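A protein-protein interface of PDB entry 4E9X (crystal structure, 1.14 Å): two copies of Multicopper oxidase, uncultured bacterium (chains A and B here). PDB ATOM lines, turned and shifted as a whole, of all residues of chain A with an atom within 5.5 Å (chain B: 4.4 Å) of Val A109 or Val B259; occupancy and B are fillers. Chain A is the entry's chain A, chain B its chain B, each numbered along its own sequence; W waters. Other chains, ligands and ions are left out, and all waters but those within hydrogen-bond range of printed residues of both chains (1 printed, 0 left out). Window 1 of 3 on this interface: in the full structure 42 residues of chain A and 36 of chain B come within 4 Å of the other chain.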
ATOM      1  N   HIS A 104      -2.537  11.758  -7.813  1.00  0.00           N
ATOM      2  CA  HIS A 104      -2.187  10.790  -8.839  1.00  0.00           C
ATOM      3  C   HIS A 104      -0.692  10.481  -8.784  1.00  0.00           C
ATOM      4  O   HIS A 104       0.077  11.322  -8.279  1.00  0.00           O
ATOM      5  CB  HIS A 104      -2.545  11.283 -10.254  1.00  0.00           C
ATOM      6  CG  HIS A 104      -1.974  12.594 -10.718  1.00  0.00           C
ATOM      7  ND1 HIS A 104      -0.697  12.757 -11.182  1.00  0.00           N
ATOM      8  CD2 HIS A 104      -2.552  13.819 -10.781  1.00  0.00           C
ATOM      9  CE1 HIS A 104      -0.514  14.049 -11.518  1.00  0.00           C
ATOM     10  NE2 HIS A 104      -1.631  14.716 -11.304  1.00  0.00           N
ATOM     11  N   CYS A 105      -0.295   9.353  -9.340  1.00  0.00           N
ATOM     12  CA  CYS A 105       1.158   9.090  -9.402  1.00  0.00           C
ATOM     13  C   CYS A 105       1.826  10.152 -10.255  1.00  0.00           C
ATOM     14  O   CYS A 105       1.230  10.697 -11.178  1.00  0.00           O
ATOM     15  CB  CYS A 105       1.347   7.683 -10.003  1.00  0.00           C
ATOM     16  SG  CYS A 105       3.080   7.164  -9.944  1.00  0.00           S
ATOM     17  N   HIS A 106       3.111  10.406  -9.989  1.00  0.00           N
ATOM     18  CA  HIS A 106       3.891  11.286 -10.845  1.00  0.00           C
ATOM     19  C   HIS A 106       5.169  10.631 -11.379  1.00  0.00           C
ATOM     20  O   HIS A 106       6.087  11.324 -11.818  1.00  0.00           O
ATOM     21  CB  HIS A 106       4.205  12.607 -10.110  1.00  0.00           C
ATOM     22  CG  HIS A 106       4.083  13.822 -10.970  1.00  0.00           C
ATOM     23  ND1 HIS A 106       4.973  14.086 -11.982  1.00  0.00           N
ATOM     24  CD2 HIS A 106       3.201  14.852 -10.963  1.00  0.00           C
ATOM     25  CE1 HIS A 106       4.625  15.210 -12.570  1.00  0.00           C
ATOM     26  NE2 HIS A 106       3.559  15.714 -11.979  1.00  0.00           N
ATOM     27  N   VAL A 107       5.219   9.300 -11.375  1.00  0.00           N
ATOM     28  CA  VAL A 107       6.243   8.500 -12.001  1.00  0.00           C
ATOM     29  C   VAL A 107       5.652   7.951 -13.336  1.00  0.00           C
ATOM     30  O   VAL A 107       4.508   7.450 -13.333  1.00  0.00           O
ATOM     31  CB  VAL A 107       6.649   7.312 -11.121  1.00  0.00           C
ATOM     32  CG1 VAL A 107       7.585   6.388 -11.909  1.00  0.00           C
ATOM     33  CG2 VAL A 107       7.275   7.750  -9.815  1.00  0.00           C
ATOM     34  N   ASN A 108       6.435   8.009 -14.384  1.00  0.00           N
ATOM     35  CA  ASN A 108       6.014   7.395 -15.646  1.00  0.00           C
ATOM     36  C   ASN A 108       4.588   7.786 -16.017  1.00  0.00           C
ATOM     37  O   ASN A 108       3.736   6.947 -16.342  1.00  0.00           O
ATOM     38  CB  ASN A 108       6.168   5.864 -15.473  1.00  0.00           C
ATOM     39  CG  ASN A 108       7.612   5.376 -15.528  1.00  0.00           C
ATOM     40  OD1 ASN A 108       8.479   6.127 -16.034  1.00  0.00           O
ATOM     41  ND2 ASN A 108       8.018   4.170 -15.094  1.00  0.00           N
ATOM     42  N   VAL A 109       4.227   9.046 -15.843  1.00  0.00           N
ATOM     43  CA  VAL A 109       2.816   9.445 -15.841  1.00  0.00           C
ATOM     44  C   VAL A 109       2.025   9.123 -17.099  1.00  0.00           C
ATOM     45  O   VAL A 109       0.826   8.857 -17.007  1.00  0.00           O
ATOM     46  CB  VAL A 109       2.659  10.953 -15.540  1.00  0.00           C
ATOM     47  CG1 VAL A 109       3.399  11.233 -14.226  1.00  0.00           C
ATOM     48  CG2 VAL A 109       3.102  11.878 -16.640  1.00  0.00           C
ATOM     49  N   ASN A 110       2.667   9.180 -18.266  1.00  0.00           N
ATOM     50  CA  ASN A 110       1.962   8.846 -19.508  1.00  0.00           C
ATOM     51  C   ASN A 110       1.320   7.481 -19.402  1.00  0.00           C
ATOM     52  O   ASN A 110       0.207   7.281 -19.885  1.00  0.00           O
ATOM     53  CB  ASN A 110       2.905   8.947 -20.718  1.00  0.00           C
ATOM     54  CG  ASN A 110       4.110   8.041 -20.651  1.00  0.00           C
ATOM     55  OD1 ASN A 110       4.939   8.217 -19.742  1.00  0.00           O
ATOM     56  ND2 ASN A 110       4.186   7.072 -21.525  1.00  0.00           N
ATOM     57  N   GLU A 111       1.999   6.527 -18.755  1.00  0.00           N
ATOM     58  CA  GLU A 111       1.420   5.207 -18.587  1.00  0.00           C
ATOM     59  C   GLU A 111       0.638   5.112 -17.299  1.00  0.00           C
ATOM     60  O   GLU A 111      -0.520   4.635 -17.273  1.00  0.00           O
ATOM     61  CB  GLU A 111       2.527   4.125 -18.614  1.00  0.00           C
ATOM     62  CG  GLU A 111       1.925   2.736 -18.432  1.00  0.00           C
ATOM     63  CD  GLU A 111       2.861   1.607 -18.082  1.00  0.00           C
ATOM     64  OE1 GLU A 111       4.092   1.796 -18.126  1.00  0.00           O
ATOM     65  OE2 GLU A 111       2.301   0.515 -17.742  1.00  0.00           O
ATOM     66  N   HIS A 112       1.237   5.502 -16.147  1.00  0.00           N
ATOM     67  CA  HIS A 112       0.615   5.215 -14.863  1.00  0.00           C
ATOM     68  C   HIS A 112      -0.697   5.982 -14.690  1.00  0.00           C
ATOM     69  O   HIS A 112      -1.663   5.418 -14.168  1.00  0.00           O
ATOM     70  CB  HIS A 112       1.621   5.500 -13.721  1.00  0.00           C
ATOM     71  CG  HIS A 112       2.719   4.472 -13.629  1.00  0.00           C
ATOM     72  ND1 HIS A 112       3.462   4.330 -12.458  1.00  0.00           N
ATOM     73  CD2 HIS A 112       3.203   3.609 -14.560  1.00  0.00           C
ATOM     74  CE1 HIS A 112       4.367   3.381 -12.670  1.00  0.00           C
ATOM     75  NE2 HIS A 112       4.230   2.940 -13.912  1.00  0.00           N
ATOM     76  N   VAL A 113      -0.695   7.269 -15.074  1.00  0.00           N
ATOM     77  CA  VAL A 113      -1.896   8.081 -14.987  1.00  0.00           C
ATOM     78  C   VAL A 113      -2.727   7.860 -16.235  1.00  0.00           C
ATOM     79  O   VAL A 113      -3.956   7.759 -16.152  1.00  0.00           O
ATOM     80  CB  VAL A 113      -1.596   9.580 -14.757  1.00  0.00           C
ATOM     81  CG1 VAL A 113      -2.873  10.386 -14.697  1.00  0.00           C
ATOM     82  CG2 VAL A 113      -0.775   9.721 -13.462  1.00  0.00           C
ATOM     83  N   GLY A 114      -2.098   7.715 -17.390  1.00  0.00           N
ATOM     84  CA  GLY A 114      -2.877   7.593 -18.644  1.00  0.00           C
ATOM     85  C   GLY A 114      -3.664   6.283 -18.729  1.00  0.00           C
ATOM     86  O   GLY A 114      -4.830   6.315 -19.189  1.00  0.00           O
ATOM     87  N   ASP B 253       3.004  20.618 -19.293  1.00  0.00           N
ATOM     88  CA  ASP B 253       1.810  20.172 -20.020  1.00  0.00           C
ATOM     89  C   ASP B 253       1.276  18.904 -19.351  1.00  0.00           C
ATOM     90  O   ASP B 253       2.049  17.938 -19.163  1.00  0.00           O
ATOM     91  CB  ASP B 253       2.199  19.916 -21.469  1.00  0.00           C
ATOM     92  CG  ASP B 253       1.075  19.567 -22.406  1.00  0.00           C
ATOM     93  OD1 ASP B 253      -0.086  19.344 -21.953  1.00  0.00           O
ATOM     94  OD2 ASP B 253       1.389  19.507 -23.635  1.00  0.00           O
ATOM     95  N   VAL B 255      -1.140  16.997 -20.549  1.00  0.00           N
ATOM     96  CA  VAL B 255      -1.667  15.984 -21.488  1.00  0.00           C
ATOM     97  C   VAL B 255      -0.697  14.809 -21.425  1.00  0.00           C
ATOM     98  O   VAL B 255       0.498  15.010 -21.743  1.00  0.00           O
ATOM     99  CB  VAL B 255      -1.804  16.547 -22.922  1.00  0.00           C
ATOM    100  CG1 VAL B 255      -2.142  15.410 -23.889  1.00  0.00           C
ATOM    101  CG2 VAL B 255      -2.824  17.682 -22.954  1.00  0.00           C
ATOM    102  N   ASP B 256      -1.166  13.607 -21.058  1.00  0.00           N
ATOM    103  CA  ASP B 256      -0.319  12.464 -20.682  1.00  0.00           C
ATOM    104  C   ASP B 256       0.679  12.079 -21.748  1.00  0.00           C
ATOM    105  O   ASP B 256       1.869  11.860 -21.425  1.00  0.00           O
ATOM    106  CB  ASP B 256      -1.218  11.280 -20.270  1.00  0.00           C
ATOM    107  CG  ASP B 256      -2.146  11.667 -19.096  1.00  0.00           C
ATOM    108  OD1 ASP B 256      -2.651  12.785 -18.841  1.00  0.00           O
ATOM    109  OD2 ASP B 256      -2.459  10.734 -18.290  1.00  0.00           O
ATOM    110  N   THR B 257       0.235  12.040 -22.992  1.00  0.00           N
ATOM    111  CA  THR B 257       1.147  11.655 -24.075  1.00  0.00           C
ATOM    112  C   THR B 257       2.184  12.710 -24.370  1.00  0.00           C
ATOM    113  O   THR B 257       3.171  12.404 -25.074  1.00  0.00           O
ATOM    114  CB  THR B 257       0.381  11.322 -25.403  1.00  0.00           C
ATOM    115  OG1 THR B 257      -0.475  12.453 -25.660  1.00  0.00           O
ATOM    116  CG2 THR B 257      -0.487  10.105 -25.252  1.00  0.00           C
ATOM    117  N   HIS B 258       2.034  13.941 -23.942  1.00  0.00           N
ATOM    118  CA  HIS B 258       2.957  15.025 -24.286  1.00  0.00           C
ATOM    119  C   HIS B 258       4.169  15.064 -23.383  1.00  0.00           C
ATOM    120  O   HIS B 258       5.106  15.780 -23.759  1.00  0.00           O
ATOM    121  CB  HIS B 258       2.244  16.398 -24.178  1.00  0.00           C
ATOM    122  CG  HIS B 258       1.177  16.515 -25.252  1.00  0.00           C
ATOM    123  ND1 HIS B 258       0.499  17.689 -25.442  1.00  0.00           N
ATOM    124  CD2 HIS B 258       0.707  15.638 -26.163  1.00  0.00           C
ATOM    125  CE1 HIS B 258      -0.341  17.549 -26.447  1.00  0.00           C
ATOM    126  NE2 HIS B 258      -0.254  16.289 -26.903  1.00  0.00           N
ATOM    127  N   VAL B 259       4.173  14.314 -22.281  1.00  0.00           N
ATOM    128  CA  VAL B 259       5.403  14.322 -21.471  1.00  0.00           C
ATOM    129  C   VAL B 259       6.202  13.071 -21.834  1.00  0.00           C
ATOM    130  O   VAL B 259       6.729  12.323 -21.024  1.00  0.00           O
ATOM    131  CB  VAL B 259       5.144  14.436 -19.976  1.00  0.00           C
ATOM    132  CG1 VAL B 259       4.695  15.870 -19.650  1.00  0.00           C
ATOM    133  CG2 VAL B 259       4.104  13.436 -19.508  1.00  0.00           C
ATOM    134  N   THR B 260       6.314  12.846 -23.127  1.00  0.00           N
ATOM    135  CA  THR B 260       7.124  11.807 -23.735  1.00  0.00           C
ATOM    136  C   THR B 260       7.984  12.439 -24.835  1.00  0.00           C
ATOM    137  O   THR B 260       7.725  13.585 -25.242  1.00  0.00           O
ATOM    138  CB  THR B 260       6.306  10.658 -24.346  1.00  0.00           C
ATOM    139  OG1 THR B 260       5.505  11.126 -25.464  1.00  0.00           O
ATOM    140  CG2 THR B 260       5.389  10.061 -23.302  1.00  0.00           C
ATOM    141  N   LYS B 264       9.587   7.682 -25.214  1.00  0.00           N
ATOM    142  CA  LYS B 264      10.339   7.594 -23.966  1.00  0.00           C
ATOM    143  C   LYS B 264       9.796   8.642 -22.978  1.00  0.00           C
ATOM    144  O   LYS B 264       9.290   9.697 -23.412  1.00  0.00           O
ATOM    145  CB  LYS B 264      11.846   7.811 -24.250  1.00  0.00           C
ATOM    146  CG  LYS B 264      12.469   7.061 -25.411  1.00  0.00           C
ATOM    147  CD  LYS B 264      13.946   7.216 -25.673  1.00  0.00           C
ATOM    148  CE  LYS B 264      14.393   8.625 -26.028  1.00  0.00           C
ATOM    149  NZ  LYS B 264      13.706   9.248 -27.190  1.00  0.00           N
ATOM    150  N   HIS B 265       9.855   8.468 -21.661  1.00  0.00           N
ATOM    151  CA  HIS B 265       9.420   9.417 -20.633  1.00  0.00           C
ATOM    152  C   HIS B 265      10.566   9.567 -19.645  1.00  0.00           C
ATOM    153  O   HIS B 265      11.226   8.557 -19.393  1.00  0.00           O
ATOM    154  CB  HIS B 265       8.165   8.954 -19.886  1.00  0.00           C
ATOM    155  CG  HIS B 265       7.766   9.735 -18.645  1.00  0.00           C
ATOM    156  ND1 HIS B 265       6.872  10.799 -18.686  1.00  0.00           N
ATOM    157  CD2 HIS B 265       8.109   9.649 -17.319  1.00  0.00           C
ATOM    158  CE1 HIS B 265       6.724  11.293 -17.443  1.00  0.00           C
ATOM    159  NE2 HIS B 265       7.456  10.625 -16.567  1.00  0.00           N
ATOM    160  N   PRO B 266      10.814  10.735 -19.082  1.00  0.00           N
ATOM    161  CA  PRO B 266      10.071  11.964 -19.364  1.00  0.00           C
ATOM    162  C   PRO B 266      10.635  12.727 -20.541  1.00  0.00           C
ATOM    163  O   PRO B 266      11.756  12.558 -20.974  1.00  0.00           O
ATOM    164  CB  PRO B 266      10.309  12.791 -18.092  1.00  0.00           C
ATOM    165  CG  PRO B 266      11.679  12.377 -17.675  1.00  0.00           C
ATOM    166  CD  PRO B 266      11.812  10.921 -18.021  1.00  0.00           C
ATOM    167  N   GLY B 267       9.795  13.617 -21.037  1.00  0.00           N
ATOM    168  CA  GLY B 267      10.165  14.481 -22.169  1.00  0.00           C
ATOM    169  C   GLY B 267       9.075  15.549 -22.234  1.00  0.00           C
ATOM    170  O   GLY B 267       8.112  15.515 -21.436  1.00  0.00           O
ATOM    171  N   ILE B 270       8.127  20.688 -20.192  1.00  0.00           N
ATOM    172  CA  ILE B 270       8.311  20.635 -18.760  1.00  0.00           C
ATOM    173  C   ILE B 270       9.387  21.646 -18.370  1.00  0.00           C
ATOM    174  O   ILE B 270      10.474  21.645 -18.978  1.00  0.00           O
ATOM    175  CB  ILE B 270       8.779  19.238 -18.279  1.00  0.00           C
ATOM    176  CG1 ILE B 270       7.862  18.086 -18.707  1.00  0.00           C
ATOM    177  CG2 ILE B 270       9.024  19.235 -16.748  1.00  0.00           C
ATOM    178  CD1 ILE B 270       8.406  16.699 -18.372  1.00  0.00           C
HETATM  179  O   HOH W   1       9.034   9.348 -13.782  1.00  0.00           O
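The backbone carbonyl oxygen of Thr B257 is in hydrogen-bond range of the side-chain hydroxyl of Thr B260, 2.7 Å away. O of Val B259 is in hydrogen-bond range of N of Gly B267. The backbone carbonyl oxygen (O) of Val A109 is in hydrogen-bond range of the backbone NH (N) of Gly A114, 3.2 Å away. The backbone carbonyl oxygen (O) of Val B259 is in hydrogen-bond range of a ring nitrogen (ND1) of His B265, at 2.8 Å.
The side-chain carboxylate of Asp B256 sits at hydrogen-bond distance from the backbone NH of Gly A114, at 3.2 Å. The side-chain amide oxygen of Asn A110 lies close to a ring nitrogen (ND1) of His B265 (3.4 Å).
Of the printed residues of chain B, Val A109 touches Asp B256, Val B259 and His B265. Of chain A, only Val A109 comes within 4 Å of Val B259. Printed residues of chain A within 4 Å of Asp B256: Val A109 (3.995 Å), Asn A110 (3.2 Å), Val A113 (3.5 Å) and Gly A114 (3.2 Å). Printed residues of chain B within 4 Å of Val A113: Asp B256. Thr B257 touches none of the printed residues of chain A. Asp B253 touches none of the printed residues of chain A.
Printed residues of chain A that touch a printed residue of chain B: Asn A108, Val A109, Asn A110, Val A113 and Gly A114. Of the 12 printed residues of chain B, 4 touch a printed residue of chain A. Printed residues of chain B that touch a printed residue of chain A: Asp B256, Val B259, Thr B260 and His B265. Hydrophobic or aromatic side chains of chain B within 4 Å of the printed part of chain A: Val B259 and His B265. Along chain B the printed residues that touch a printed residue of chain A span positions 256 to 265.
No position is printed for both chains.
Water W1 lies within hydrogen-bond range of the backbone NH of Asn A108 (3.0 Å) and a ring nitrogen (NE2) of His B265 (3.4 Å).
Asn A108 touches His B265 (CA to CD2, 3.5 Å). Val A109 touches Asp B256 (O to OD2, 3.995 Å). Val A109 touches Val B259. Val A109 touches His B265. Asn A110 touches Asp B256 (CB to O, 3.2 Å). CG of Asn A110 touches CG2 of Thr B260, 3.6 Å away. Asp B256 touches Val A113.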
